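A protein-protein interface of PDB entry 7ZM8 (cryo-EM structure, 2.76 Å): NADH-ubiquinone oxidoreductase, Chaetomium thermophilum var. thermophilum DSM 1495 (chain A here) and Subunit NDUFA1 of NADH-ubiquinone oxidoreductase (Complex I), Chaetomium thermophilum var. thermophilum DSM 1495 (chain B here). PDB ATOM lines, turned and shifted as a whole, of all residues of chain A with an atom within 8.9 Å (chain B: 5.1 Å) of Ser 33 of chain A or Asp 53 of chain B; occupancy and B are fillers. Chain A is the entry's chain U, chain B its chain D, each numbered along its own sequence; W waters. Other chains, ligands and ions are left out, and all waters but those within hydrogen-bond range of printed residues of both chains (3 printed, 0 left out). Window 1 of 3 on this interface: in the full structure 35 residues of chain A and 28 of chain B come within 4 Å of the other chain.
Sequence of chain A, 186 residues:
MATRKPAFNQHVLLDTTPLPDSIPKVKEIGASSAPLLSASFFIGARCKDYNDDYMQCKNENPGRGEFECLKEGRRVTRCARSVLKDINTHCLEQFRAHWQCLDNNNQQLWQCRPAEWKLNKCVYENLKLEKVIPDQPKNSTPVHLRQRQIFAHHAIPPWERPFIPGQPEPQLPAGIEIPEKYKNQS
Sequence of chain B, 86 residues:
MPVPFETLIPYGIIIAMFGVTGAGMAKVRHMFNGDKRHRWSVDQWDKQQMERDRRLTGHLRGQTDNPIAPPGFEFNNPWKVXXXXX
The guanidinium group (NH2) of Arg 52 of chain B sits at hydrogen-bond distance from the backbone carbonyl oxygen (O) of Ile 29 of chain A (2.9 Å). The side-chain carboxylate of Asp 103 of chain A sits close to the side-chain amide nitrogen of Gln 63 of chain B. O of Ala 31 of chain A sits at hydrogen-bond distance from NH1 of Arg 52 of chain B. The backbone carbonyl oxygen of Asp 103 of chain A lies within hydrogen-bond range of the guanidinium group of Arg 61 of chain B, 3.0 Å away. The backbone NH (N) of Ala 34 of chain A is in hydrogen-bond range of the side-chain amide oxygen (OE1) of Gln 63 of chain B (3.2 Å). OD1 of Asp 53 of chain B is in hydrogen-bond range of N of Ser 33 of chain A.
Water W1 lies within hydrogen-bond range of O of Gln 49 of chain B (2.8 Å), OD1 of Asp 53 of chain B (3.0 Å) and N of Ser 33 of chain A (3.2 Å). Water W3 lies within hydrogen-bond range of NE2 of Gln 107 of chain A (2.8 Å), NE2 of Gln 63 of chain B (3.4 Å) and OD1 of Asp 103 of chain A (3.5 Å). Water W2 bridges NE2 of Gln 49 of chain B and OG of Ser 33 of chain A.
Printed residues of chain B that touch a printed residue of chain A: Gln 49, Arg 52, Asp 53, Leu 56, Arg 61, Gly 62 and Gln 63. Hydrophobic or aromatic side chains of chain A within 4 Å of the printed part of chain B: Ile 29, Ala 34, Pro 35, Leu 36 and Trp 99. Along chain A the printed residues that touch a printed residue of chain B span positions 29 to 107. Among the printed residues, 18 pairs touch across the chains.
Of the printed residues of chain B, Ser 32 of chain A touches Asp 53 (3.2 Å), Leu 56 (3.97 Å), Gly 62 (3.7 Å) and Gln 63 (3.1 Å). Ser 33 of chain A touches just these residues of chain B: Gln 49, Asp 53 and Gln 63. Printed residues of chain B within 4 Å of Pro 35 of chain A: Gln 63 (3.2 Å). Of the printed residues of chain B, Gln 107 of chain A touches Gln 63 (3.8 Å). Asp 53 of chain B touches two residues of chain A. Of chain A, only Ser 32 (3.7 Å) comes within 4 Å of Gly 62 of chain B. The nearest residue of chain B that does not touch Ser 33 of chain A is Arg 52 of chain B (4.9 Å). The nearest residue of chain A that does not touch Asp 53 of chain B is Gln 107 of chain A (5.0 Å). The nearest printed residue of chain B that does not touch Ala 31 of chain A is Asp 53 of chain B (5.7 Å).
O of Asp 53 of chain B sits at hydrogen-bond distance from OG1 of Thr 57 of chain B, 2.9 Å away. ND1 of His 59 of chain B lies close to N of Arg 61 of chain B, at 3.5 Å. The side-chain amide oxygen (OE1) of Gln 107 of chain A sits at hydrogen-bond distance from the side-chain hydroxyl (OG) of Ser 33 of chain A. The backbone carbonyl oxygen (O) of Leu 102 of chain A is in hydrogen-bond range of the backbone NH (N) of Gln 107 of chain A, 2.9 Å away. N of Trp 99 of chain A sits close to OG of Ser 38 of chain A (3.4 Å).
Gly 30 of chain A touches Leu 56 of chain B (CA to CD2, 3.6 Å). CD1 of Leu 56 of chain B touches O of Ala 31 of chain A, at 3.4 Å. Ser 32 of chain A touches Asp 53 of chain B. Ser 32 of chain A touches Leu 56 of chain B (OG to CD1, 3.97 Å). Gln 49 of chain B touches Ser 33 of chain A. N of Ser 33 of chain A touches OE1 of Gln 63 of chain B, at 3.7 Å. Gln 63 of chain B touches Pro 35 of chain A. Arg 52 of chain B touches Leu 36 of chain A. Trp 99 of chain A touches Gln 63 of chain B (CZ3 to CB, 3.5 Å). Gln 107 of chain A touches Gln 63 of chain B (NE2 to NE2, 3.8 Å).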
ATOM      1  N   ILE A  29      24.440   1.192 -16.700  1.00  0.00           N
ATOM      2  CA  ILE A  29      23.139   1.479 -17.369  1.00  0.00           C
ATOM      3  C   ILE A  29      23.140   0.911 -18.797  1.00  0.00           C
ATOM      4  O   ILE A  29      24.170   1.029 -19.476  1.00  0.00           O
ATOM      5  CB  ILE A  29      22.843   2.992 -17.317  1.00  0.00           C
ATOM      6  CG1 ILE A  29      22.360   3.423 -15.932  1.00  0.00           C
ATOM      7  CG2 ILE A  29      21.878   3.416 -18.412  1.00  0.00           C
ATOM      8  CD1 ILE A  29      22.907   4.752 -15.489  1.00  0.00           C
ATOM      9  N   GLY A  30      22.046   0.278 -19.216  1.00  0.00           N
ATOM     10  CA  GLY A  30      21.912  -0.297 -20.536  1.00  0.00           C
ATOM     11  C   GLY A  30      20.970   0.423 -21.467  1.00  0.00           C
ATOM     12  O   GLY A  30      20.593  -0.146 -22.500  1.00  0.00           O
ATOM     13  N   ALA A  31      20.552   1.639 -21.139  1.00  0.00           N
ATOM     14  CA  ALA A  31      19.688   2.407 -22.013  1.00  0.00           C
ATOM     15  C   ALA A  31      20.516   3.135 -23.055  1.00  0.00           C
ATOM     16  O   ALA A  31      21.626   3.596 -22.779  1.00  0.00           O
ATOM     17  CB  ALA A  31      18.860   3.408 -21.213  1.00  0.00           C
ATOM     18  N   SER A  32      19.964   3.240 -24.256  1.00  0.00           N
ATOM     19  CA  SER A  32      20.648   3.889 -25.362  1.00  0.00           C
ATOM     20  C   SER A  32      20.471   5.400 -25.278  1.00  0.00           C
ATOM     21  O   SER A  32      19.910   5.941 -24.324  1.00  0.00           O
ATOM     22  CB  SER A  32      20.149   3.330 -26.685  1.00  0.00           C
ATOM     23  OG  SER A  32      20.516   1.979 -26.817  1.00  0.00           O
ATOM     24  N   SER A  33      20.951   6.094 -26.310  1.00  0.00           N
ATOM     25  CA  SER A  33      20.969   7.549 -26.299  1.00  0.00           C
ATOM     26  C   SER A  33      19.563   8.131 -26.270  1.00  0.00           C
ATOM     27  O   SER A  33      19.306   9.106 -25.557  1.00  0.00           O
ATOM     28  CB  SER A  33      21.740   8.060 -27.510  1.00  0.00           C
ATOM     29  OG  SER A  33      21.404   9.399 -27.793  1.00  0.00           O
ATOM     30  N   ALA A  34      18.639   7.550 -27.025  1.00  0.00           N
ATOM     31  CA  ALA A  34      17.317   8.147 -27.140  1.00  0.00           C
ATOM     32  C   ALA A  34      16.466   7.876 -25.902  1.00  0.00           C
ATOM     33  O   ALA A  34      15.812   8.804 -25.412  1.00  0.00           O
ATOM     34  CB  ALA A  34      16.610   7.672 -28.412  1.00  0.00           C
ATOM     35  N   PRO A  35      16.424   6.646 -25.364  1.00  0.00           N
ATOM     36  CA  PRO A  35      15.753   6.463 -24.068  1.00  0.00           C
ATOM     37  C   PRO A  35      16.321   7.316 -22.947  1.00  0.00           C
ATOM     38  O   PRO A  35      15.569   7.743 -22.067  1.00  0.00           O
ATOM     39  CB  PRO A  35      15.945   4.968 -23.798  1.00  0.00           C
ATOM     40  CG  PRO A  35      15.972   4.375 -25.116  1.00  0.00           C
ATOM     41  CD  PRO A  35      16.700   5.340 -25.989  1.00  0.00           C
ATOM     42  N   LEU A  36      17.630   7.564 -22.933  1.00  0.00           N
ATOM     43  CA  LEU A  36      18.204   8.402 -21.882  1.00  0.00           C
ATOM     44  C   LEU A  36      17.729   9.843 -21.996  1.00  0.00           C
ATOM     45  O   LEU A  36      17.535  10.519 -20.981  1.00  0.00           O
ATOM     46  CB  LEU A  36      19.728   8.340 -21.925  1.00  0.00           C
ATOM     47  CG  LEU A  36      20.360   7.110 -21.280  1.00  0.00           C
ATOM     48  CD1 LEU A  36      21.872   7.230 -21.289  1.00  0.00           C
ATOM     49  CD2 LEU A  36      19.840   6.902 -19.876  1.00  0.00           C
ATOM     50  N   LEU A  37      17.548  10.338 -23.217  1.00  0.00           N
ATOM     51  CA  LEU A  37      17.102  11.711 -23.391  1.00  0.00           C
ATOM     52  C   LEU A  37      15.615  11.868 -23.097  1.00  0.00           C
ATOM     53  O   LEU A  37      15.182  12.941 -22.671  1.00  0.00           O
ATOM     54  CB  LEU A  37      17.436  12.182 -24.803  1.00  0.00           C
ATOM     55  CG  LEU A  37      17.104  13.624 -25.165  1.00  0.00           C
ATOM     56  CD1 LEU A  37      18.089  14.558 -24.508  1.00  0.00           C
ATOM     57  CD2 LEU A  37      17.126  13.783 -26.664  1.00  0.00           C
ATOM     58  N   SER A  38      14.817  10.825 -23.325  1.00  0.00           N
ATOM     59  CA  SER A  38      13.414  10.876 -22.926  1.00  0.00           C
ATOM     60  C   SER A  38      13.277  11.000 -21.419  1.00  0.00           C
ATOM     61  O   SER A  38      12.425  11.746 -20.927  1.00  0.00           O
ATOM     62  CB  SER A  38      12.675   9.636 -23.416  1.00  0.00           C
ATOM     63  OG  SER A  38      12.391   9.720 -24.793  1.00  0.00           O
ATOM     64  N   ALA A  39      14.102  10.272 -20.675  1.00  0.00           N
ATOM     65  CA  ALA A  39      14.031  10.242 -19.225  1.00  0.00           C
ATOM     66  C   ALA A  39      15.040  11.168 -18.570  1.00  0.00           C
ATOM     67  O   ALA A  39      15.199  11.121 -17.351  1.00  0.00           O
ATOM     68  CB  ALA A  39      14.226   8.814 -18.726  1.00  0.00           C
ATOM     69  N   SER A  40      15.714  12.017 -19.349  1.00  0.00           N
ATOM     70  CA  SER A  40      16.781  12.848 -18.803  1.00  0.00           C
ATOM     71  C   SER A  40      16.258  13.816 -17.754  1.00  0.00           C
ATOM     72  O   SER A  40      16.902  14.034 -16.725  1.00  0.00           O
ATOM     73  CB  SER A  40      17.483  13.607 -19.928  1.00  0.00           C
ATOM     74  OG  SER A  40      16.613  14.541 -20.532  1.00  0.00           O
ATOM     75  N   PHE A  95       6.579   5.832 -22.856  1.00  0.00           N
ATOM     76  CA  PHE A  95       8.019   6.049 -22.872  1.00  0.00           C
ATOM     77  C   PHE A  95       8.624   5.623 -24.199  1.00  0.00           C
ATOM     78  O   PHE A  95       9.389   6.376 -24.807  1.00  0.00           O
ATOM     79  CB  PHE A  95       8.648   5.285 -21.709  1.00  0.00           C
ATOM     80  CG  PHE A  95      10.143   5.349 -21.655  1.00  0.00           C
ATOM     81  CD1 PHE A  95      10.801   6.563 -21.572  1.00  0.00           C
ATOM     82  CD2 PHE A  95      10.892   4.192 -21.635  1.00  0.00           C
ATOM     83  CE1 PHE A  95      12.171   6.614 -21.502  1.00  0.00           C
ATOM     84  CE2 PHE A  95      12.260   4.241 -21.559  1.00  0.00           C
ATOM     85  CZ  PHE A  95      12.900   5.451 -21.496  1.00  0.00           C
ATOM     86  N   TRP A  99      10.673   8.021 -27.165  1.00  0.00           N
ATOM     87  CA  TRP A  99      12.059   7.964 -27.614  1.00  0.00           C
ATOM     88  C   TRP A  99      12.206   7.359 -28.997  1.00  0.00           C
ATOM     89  O   TRP A  99      13.186   7.661 -29.680  1.00  0.00           O
ATOM     90  CB  TRP A  99      12.955   7.223 -26.606  1.00  0.00           C
ATOM     91  CG  TRP A  99      12.683   5.775 -26.329  1.00  0.00           C
ATOM     92  CD1 TRP A  99      12.110   5.259 -25.216  1.00  0.00           C
ATOM     93  CD2 TRP A  99      13.054   4.654 -27.143  1.00  0.00           C
ATOM     94  NE1 TRP A  99      12.068   3.896 -25.290  1.00  0.00           N
ATOM     95  CE2 TRP A  99      12.640   3.497 -26.467  1.00  0.00           C
ATOM     96  CE3 TRP A  99      13.689   4.521 -28.382  1.00  0.00           C
ATOM     97  CZ2 TRP A  99      12.826   2.226 -26.987  1.00  0.00           C
ATOM     98  CZ3 TRP A  99      13.870   3.260 -28.896  1.00  0.00           C
ATOM     99  CH2 TRP A  99      13.444   2.128 -28.199  1.00  0.00           C
ATOM    100  N   LEU A 102      11.960  10.488 -30.993  1.00  0.00           N
ATOM    101  CA  LEU A 102      13.247  11.173 -31.019  1.00  0.00           C
ATOM    102  C   LEU A 102      14.236  10.446 -31.909  1.00  0.00           C
ATOM    103  O   LEU A 102      15.119  11.067 -32.509  1.00  0.00           O
ATOM    104  CB  LEU A 102      13.817  11.286 -29.606  1.00  0.00           C
ATOM    105  CG  LEU A 102      13.130  12.182 -28.584  1.00  0.00           C
ATOM    106  CD1 LEU A 102      13.316  11.610 -27.206  1.00  0.00           C
ATOM    107  CD2 LEU A 102      13.688  13.581 -28.646  1.00  0.00           C
ATOM    108  N   ASP A 103      14.131   9.130 -32.042  1.00  0.00           N
ATOM    109  CA  ASP A 103      15.018   8.356 -32.962  1.00  0.00           C
ATOM    110  C   ASP A 103      14.957   8.910 -34.390  1.00  0.00           C
ATOM    111  O   ASP A 103      15.989   8.893 -35.066  1.00  0.00           O
ATOM    112  CB  ASP A 103      14.594   6.894 -33.037  1.00  0.00           C
ATOM    113  CG  ASP A 103      15.110   6.054 -31.897  1.00  0.00           C
ATOM    114  OD1 ASP A 103      15.911   6.585 -31.123  1.00  0.00           O
ATOM    115  OD2 ASP A 103      14.710   4.880 -31.805  1.00  0.00           O
ATOM    116  N   ASN A 106      16.160  13.485 -35.154  1.00  0.00           N
ATOM    117  CA  ASN A 106      17.516  14.046 -34.876  1.00  0.00           C
ATOM    118  C   ASN A 106      17.690  14.145 -33.362  1.00  0.00           C
ATOM    119  O   ASN A 106      18.572  14.891 -32.923  1.00  0.00           O
ATOM    120  CB  ASN A 106      17.812  15.343 -35.642  1.00  0.00           C
ATOM    121  CG  ASN A 106      19.276  15.549 -35.960  1.00  0.00           C
ATOM    122  OD1 ASN A 106      20.013  14.591 -36.166  1.00  0.00           O
ATOM    123  ND2 ASN A 106      19.701  16.797 -36.024  1.00  0.00           N
ATOM    124  N   GLN A 107      16.895  13.399 -32.605  1.00  0.00           N
ATOM    125  CA  GLN A 107      16.944  13.473 -31.128  1.00  0.00           C
ATOM    126  C   GLN A 107      16.718  14.927 -30.729  1.00  0.00           C
ATOM    127  O   GLN A 107      17.488  15.426 -29.898  1.00  0.00           O
ATOM    128  CB  GLN A 107      18.209  12.809 -30.581  1.00  0.00           C
ATOM    129  CG  GLN A 107      18.142  11.293 -30.620  1.00  0.00           C
ATOM    130  CD  GLN A 107      19.276  10.659 -29.859  1.00  0.00           C
ATOM    131  OE1 GLN A 107      20.004  11.326 -29.132  1.00  0.00           O
ATOM    132  NE2 GLN A 107      19.431   9.357 -30.019  1.00  0.00           N
ATOM    133  N   GLN B  49      27.494   9.444 -28.234  1.00  0.00           N
ATOM    134  CA  GLN B  49      26.206   8.806 -27.871  1.00  0.00           C
ATOM    135  C   GLN B  49      25.909   7.658 -28.841  1.00  0.00           C
ATOM    136  O   GLN B  49      25.388   6.632 -28.388  1.00  0.00           O
ATOM    137  CB  GLN B  49      25.099   9.858 -27.748  1.00  0.00           C
ATOM    138  CG  GLN B  49      25.117  10.630 -26.438  1.00  0.00           C
ATOM    139  CD  GLN B  49      24.536   9.887 -25.259  1.00  0.00           C
ATOM    140  OE1 GLN B  49      24.727   8.687 -25.090  1.00  0.00           O
ATOM    141  NE2 GLN B  49      23.826  10.611 -24.411  1.00  0.00           N
ATOM    142  N   MET B  50      26.229   7.831 -30.120  1.00  0.00           N
ATOM    143  CA  MET B  50      26.024   6.767 -31.140  1.00  0.00           C
ATOM    144  C   MET B  50      27.062   5.657 -30.987  1.00  0.00           C
ATOM    145  O   MET B  50      26.719   4.512 -31.294  1.00  0.00           O
ATOM    146  CB  MET B  50      26.116   7.344 -32.550  1.00  0.00           C
ATOM    147  CG  MET B  50      24.833   8.002 -33.010  1.00  0.00           C
ATOM    148  SD  MET B  50      24.912   8.566 -34.722  1.00  0.00           S
ATOM    149  CE  MET B  50      25.815  10.100 -34.523  1.00  0.00           C
ATOM    150  N   GLU B  51      28.280   5.981 -30.555  1.00  0.00           N
ATOM    151  CA  GLU B  51      29.312   4.948 -30.300  1.00  0.00           C
ATOM    152  C   GLU B  51      28.851   4.049 -29.160  1.00  0.00           C
ATOM    153  O   GLU B  51      29.175   2.865 -29.186  1.00  0.00           O
ATOM    154  CB  GLU B  51      30.678   5.609 -30.170  1.00  0.00           C
ATOM    155  CG  GLU B  51      31.259   6.023 -31.503  1.00  0.00           C
ATOM    156  CD  GLU B  51      32.733   6.374 -31.467  1.00  0.00           C
ATOM    157  OE1 GLU B  51      33.386   6.044 -30.462  1.00  0.00           O
ATOM    158  OE2 GLU B  51      33.220   6.974 -32.444  1.00  0.00           O
ATOM    159  N   ARG B  52      28.147   4.613 -28.190  1.00  0.00           N
ATOM    160  CA  ARG B  52      27.633   3.834 -27.049  1.00  0.00           C
ATOM    161  C   ARG B  52      26.404   3.073 -27.514  1.00  0.00           C
ATOM    162  O   ARG B  52      26.090   2.060 -26.889  1.00  0.00           O
ATOM    163  CB  ARG B  52      27.414   4.757 -25.857  1.00  0.00           C
ATOM    164  CG  ARG B  52      27.033   4.049 -24.568  1.00  0.00           C
ATOM    165  CD  ARG B  52      26.704   5.058 -23.493  1.00  0.00           C
ATOM    166  NE  ARG B  52      26.257   4.354 -22.308  1.00  0.00           N
ATOM    167  CZ  ARG B  52      24.991   4.241 -21.954  1.00  0.00           C
ATOM    168  NH1 ARG B  52      24.056   4.820 -22.683  1.00  0.00           N
ATOM    169  NH2 ARG B  52      24.665   3.569 -20.867  1.00  0.00           N
ATOM    170  N   ASP B  53      25.720   3.549 -28.561  1.00  0.00           N
ATOM    171  CA  ASP B  53      24.646   2.722 -29.101  1.00  0.00           C
ATOM    172  C   ASP B  53      25.202   1.460 -29.740  1.00  0.00           C
ATOM    173  O   ASP B  53      24.595   0.390 -29.647  1.00  0.00           O
ATOM    174  CB  ASP B  53      23.838   3.510 -30.128  1.00  0.00           C
ATOM    175  CG  ASP B  53      23.040   4.628 -29.510  1.00  0.00           C
ATOM    176  OD1 ASP B  53      22.652   4.506 -28.334  1.00  0.00           O
ATOM    177  OD2 ASP B  53      22.767   5.620 -30.219  1.00  0.00           O
ATOM    178  N   ARG B  54      26.350   1.558 -30.408  1.00  0.00           N
ATOM    179  CA  ARG B  54      27.029   0.364 -30.977  1.00  0.00           C
ATOM    180  C   ARG B  54      27.569  -0.520 -29.855  1.00  0.00           C
ATOM    181  O   ARG B  54      27.667  -1.734 -30.068  1.00  0.00           O
ATOM    182  CB  ARG B  54      28.145   0.814 -31.926  1.00  0.00           C
ATOM    183  CG  ARG B  54      28.738  -0.299 -32.775  1.00  0.00           C
ATOM    184  CD  ARG B  54      29.497   0.215 -33.980  1.00  0.00           C
ATOM    185  NE  ARG B  54      30.539   1.149 -33.586  1.00  0.00           N
ATOM    186  CZ  ARG B  54      31.370   1.749 -34.427  1.00  0.00           C
ATOM    187  NH1 ARG B  54      32.282   2.586 -33.965  1.00  0.00           N
ATOM    188  NH2 ARG B  54      31.289   1.511 -35.722  1.00  0.00           N
ATOM    189  N   ARG B  55      27.889   0.059 -28.706  1.00  0.00           N
ATOM    190  CA  ARG B  55      28.362  -0.733 -27.545  1.00  0.00           C
ATOM    191  C   ARG B  55      27.218  -1.598 -27.008  1.00  0.00           C
ATOM    192  O   ARG B  55      27.486  -2.768 -26.690  1.00  0.00           O
ATOM    193  CB  ARG B  55      28.941   0.185 -26.469  1.00  0.00           C
ATOM    194  CG  ARG B  55      30.331   0.724 -26.763  1.00  0.00           C
ATOM    195  CD  ARG B  55      30.745   1.569 -25.579  1.00  0.00           C
ATOM    196  NE  ARG B  55      30.911   0.749 -24.391  1.00  0.00           N
ATOM    197  CZ  ARG B  55      31.002   1.227 -23.158  1.00  0.00           C
ATOM    198  NH1 ARG B  55      30.913   2.526 -22.947  1.00  0.00           N
ATOM    199  NH2 ARG B  55      31.164   0.407 -22.136  1.00  0.00           N
ATOM    200  N   LEU B  56      25.995  -1.066 -26.927  1.00  0.00           N
ATOM    201  CA  LEU B  56      24.874  -1.807 -26.366  1.00  0.00           C
ATOM    202  C   LEU B  56      24.222  -2.729 -27.389  1.00  0.00           C
ATOM    203  O   LEU B  56      23.794  -3.833 -27.042  1.00  0.00           O
ATOM    204  CB  LEU B  56      23.846  -0.831 -25.795  1.00  0.00           C
ATOM    205  CG  LEU B  56      24.264  -0.108 -24.514  1.00  0.00           C
ATOM    206  CD1 LEU B  56      23.520   1.199 -24.341  1.00  0.00           C
ATOM    207  CD2 LEU B  56      24.061  -0.999 -23.315  1.00  0.00           C
ATOM    208  N   THR B  57      24.131  -2.307 -28.647  1.00  0.00           N
ATOM    209  CA  THR B  57      23.392  -3.060 -29.652  1.00  0.00           C
ATOM    210  C   THR B  57      24.236  -3.580 -30.803  1.00  0.00           C
ATOM    211  O   THR B  57      23.856  -4.578 -31.415  1.00  0.00           O
ATOM    212  CB  THR B  57      22.257  -2.209 -30.241  1.00  0.00           C
ATOM    213  OG1 THR B  57      22.800  -1.271 -31.175  1.00  0.00           O
ATOM    214  CG2 THR B  57      21.502  -1.468 -29.147  1.00  0.00           C
ATOM    215  N   GLY B  58      25.358  -2.946 -31.120  1.00  0.00           N
ATOM    216  CA  GLY B  58      26.145  -3.304 -32.280  1.00  0.00           C
ATOM    217  C   GLY B  58      25.948  -2.399 -33.475  1.00  0.00           C
ATOM    218  O   GLY B  58      26.763  -2.438 -34.399  1.00  0.00           O
ATOM    219  N   HIS B  59      24.903  -1.580 -33.468  1.00  0.00           N
ATOM    220  CA  HIS B  59      24.579  -0.654 -34.541  1.00  0.00           C
ATOM    221  C   HIS B  59      24.639   0.766 -34.004  1.00  0.00           C
ATOM    222  O   HIS B  59      24.132   1.044 -32.918  1.00  0.00           O
ATOM    223  CB  HIS B  59      23.187  -0.958 -35.103  1.00  0.00           C
ATOM    224  CG  HIS B  59      22.827  -0.173 -36.326  1.00  0.00           C
ATOM    225  ND1 HIS B  59      23.724   0.659 -36.960  1.00  0.00           N
ATOM    226  CD2 HIS B  59      21.680  -0.099 -37.041  1.00  0.00           C
ATOM    227  CE1 HIS B  59      23.143   1.214 -38.007  1.00  0.00           C
ATOM    228  NE2 HIS B  59      21.902   0.772 -38.078  1.00  0.00           N
ATOM    229  N   LEU B  60      25.262   1.666 -34.773  1.00  0.00           N
ATOM    230  CA  LEU B  60      25.421   3.045 -34.324  1.00  0.00           C
ATOM    231  C   LEU B  60      24.082   3.735 -34.109  1.00  0.00           C
ATOM    232  O   LEU B  60      24.003   4.703 -33.347  1.00  0.00           O
ATOM    233  CB  LEU B  60      26.264   3.836 -35.323  1.00  0.00           C
ATOM    234  CG  LEU B  60      27.759   3.517 -35.354  1.00  0.00           C
ATOM    235  CD1 LEU B  60      28.384   3.928 -36.672  1.00  0.00           C
ATOM    236  CD2 LEU B  60      28.483   4.169 -34.188  1.00  0.00           C
ATOM    237  N   ARG B  61      23.023   3.262 -34.758  1.00  0.00           N
ATOM    238  CA  ARG B  61      21.691   3.808 -34.562  1.00  0.00           C
ATOM    239  C   ARG B  61      20.785   2.879 -33.765  1.00  0.00           C
ATOM    240  O   ARG B  61      19.590   3.159 -33.636  1.00  0.00           O
ATOM    241  CB  ARG B  61      21.046   4.135 -35.909  1.00  0.00           C
ATOM    242  CG  ARG B  61      21.890   5.016 -36.803  1.00  0.00           C
ATOM    243  CD  ARG B  61      22.003   6.430 -36.267  1.00  0.00           C
ATOM    244  NE  ARG B  61      20.725   6.949 -35.795  1.00  0.00           N
ATOM    245  CZ  ARG B  61      19.826   7.543 -36.571  1.00  0.00           C
ATOM    246  NH1 ARG B  61      18.693   7.982 -36.057  1.00  0.00           N
ATOM    247  NH2 ARG B  61      20.062   7.700 -37.861  1.00  0.00           N
ATOM    248  N   GLY B  62      21.319   1.788 -33.226  1.00  0.00           N
ATOM    249  CA  GLY B  62      20.496   0.883 -32.451  1.00  0.00           C
ATOM    250  C   GLY B  62      20.089   1.478 -31.118  1.00  0.00           C
ATOM    251  O   GLY B  62      20.819   2.253 -30.505  1.00  0.00           O
ATOM    252  N   GLN B  63      18.903   1.089 -30.657  1.00  0.00           N
ATOM    253  CA  GLN B  63      18.301   1.651 -29.457  1.00  0.00           C
ATOM    254  C   GLN B  63      17.752   0.546 -28.573  1.00  0.00           C
ATOM    255  O   GLN B  63      17.217  -0.447 -29.068  1.00  0.00           O
ATOM    256  CB  GLN B  63      17.179   2.621 -29.807  1.00  0.00           C
ATOM    257  CG  GLN B  63      17.604   3.786 -30.666  1.00  0.00           C
ATOM    258  CD  GLN B  63      18.389   4.804 -29.894  1.00  0.00           C
ATOM    259  OE1 GLN B  63      18.362   4.822 -28.674  1.00  0.00           O
ATOM    260  NE2 GLN B  63      19.100   5.662 -30.602  1.00  0.00           N
HETATM  261  O   HOH W   1      24.101   5.813 -26.051  1.00  0.00           O
HETATM  262  O   HOH W   2      21.395  12.218 -25.748  1.00  0.00           O
HETATM  263  O   HOH W   3      18.528   8.404 -32.486  1.00  0.00           O
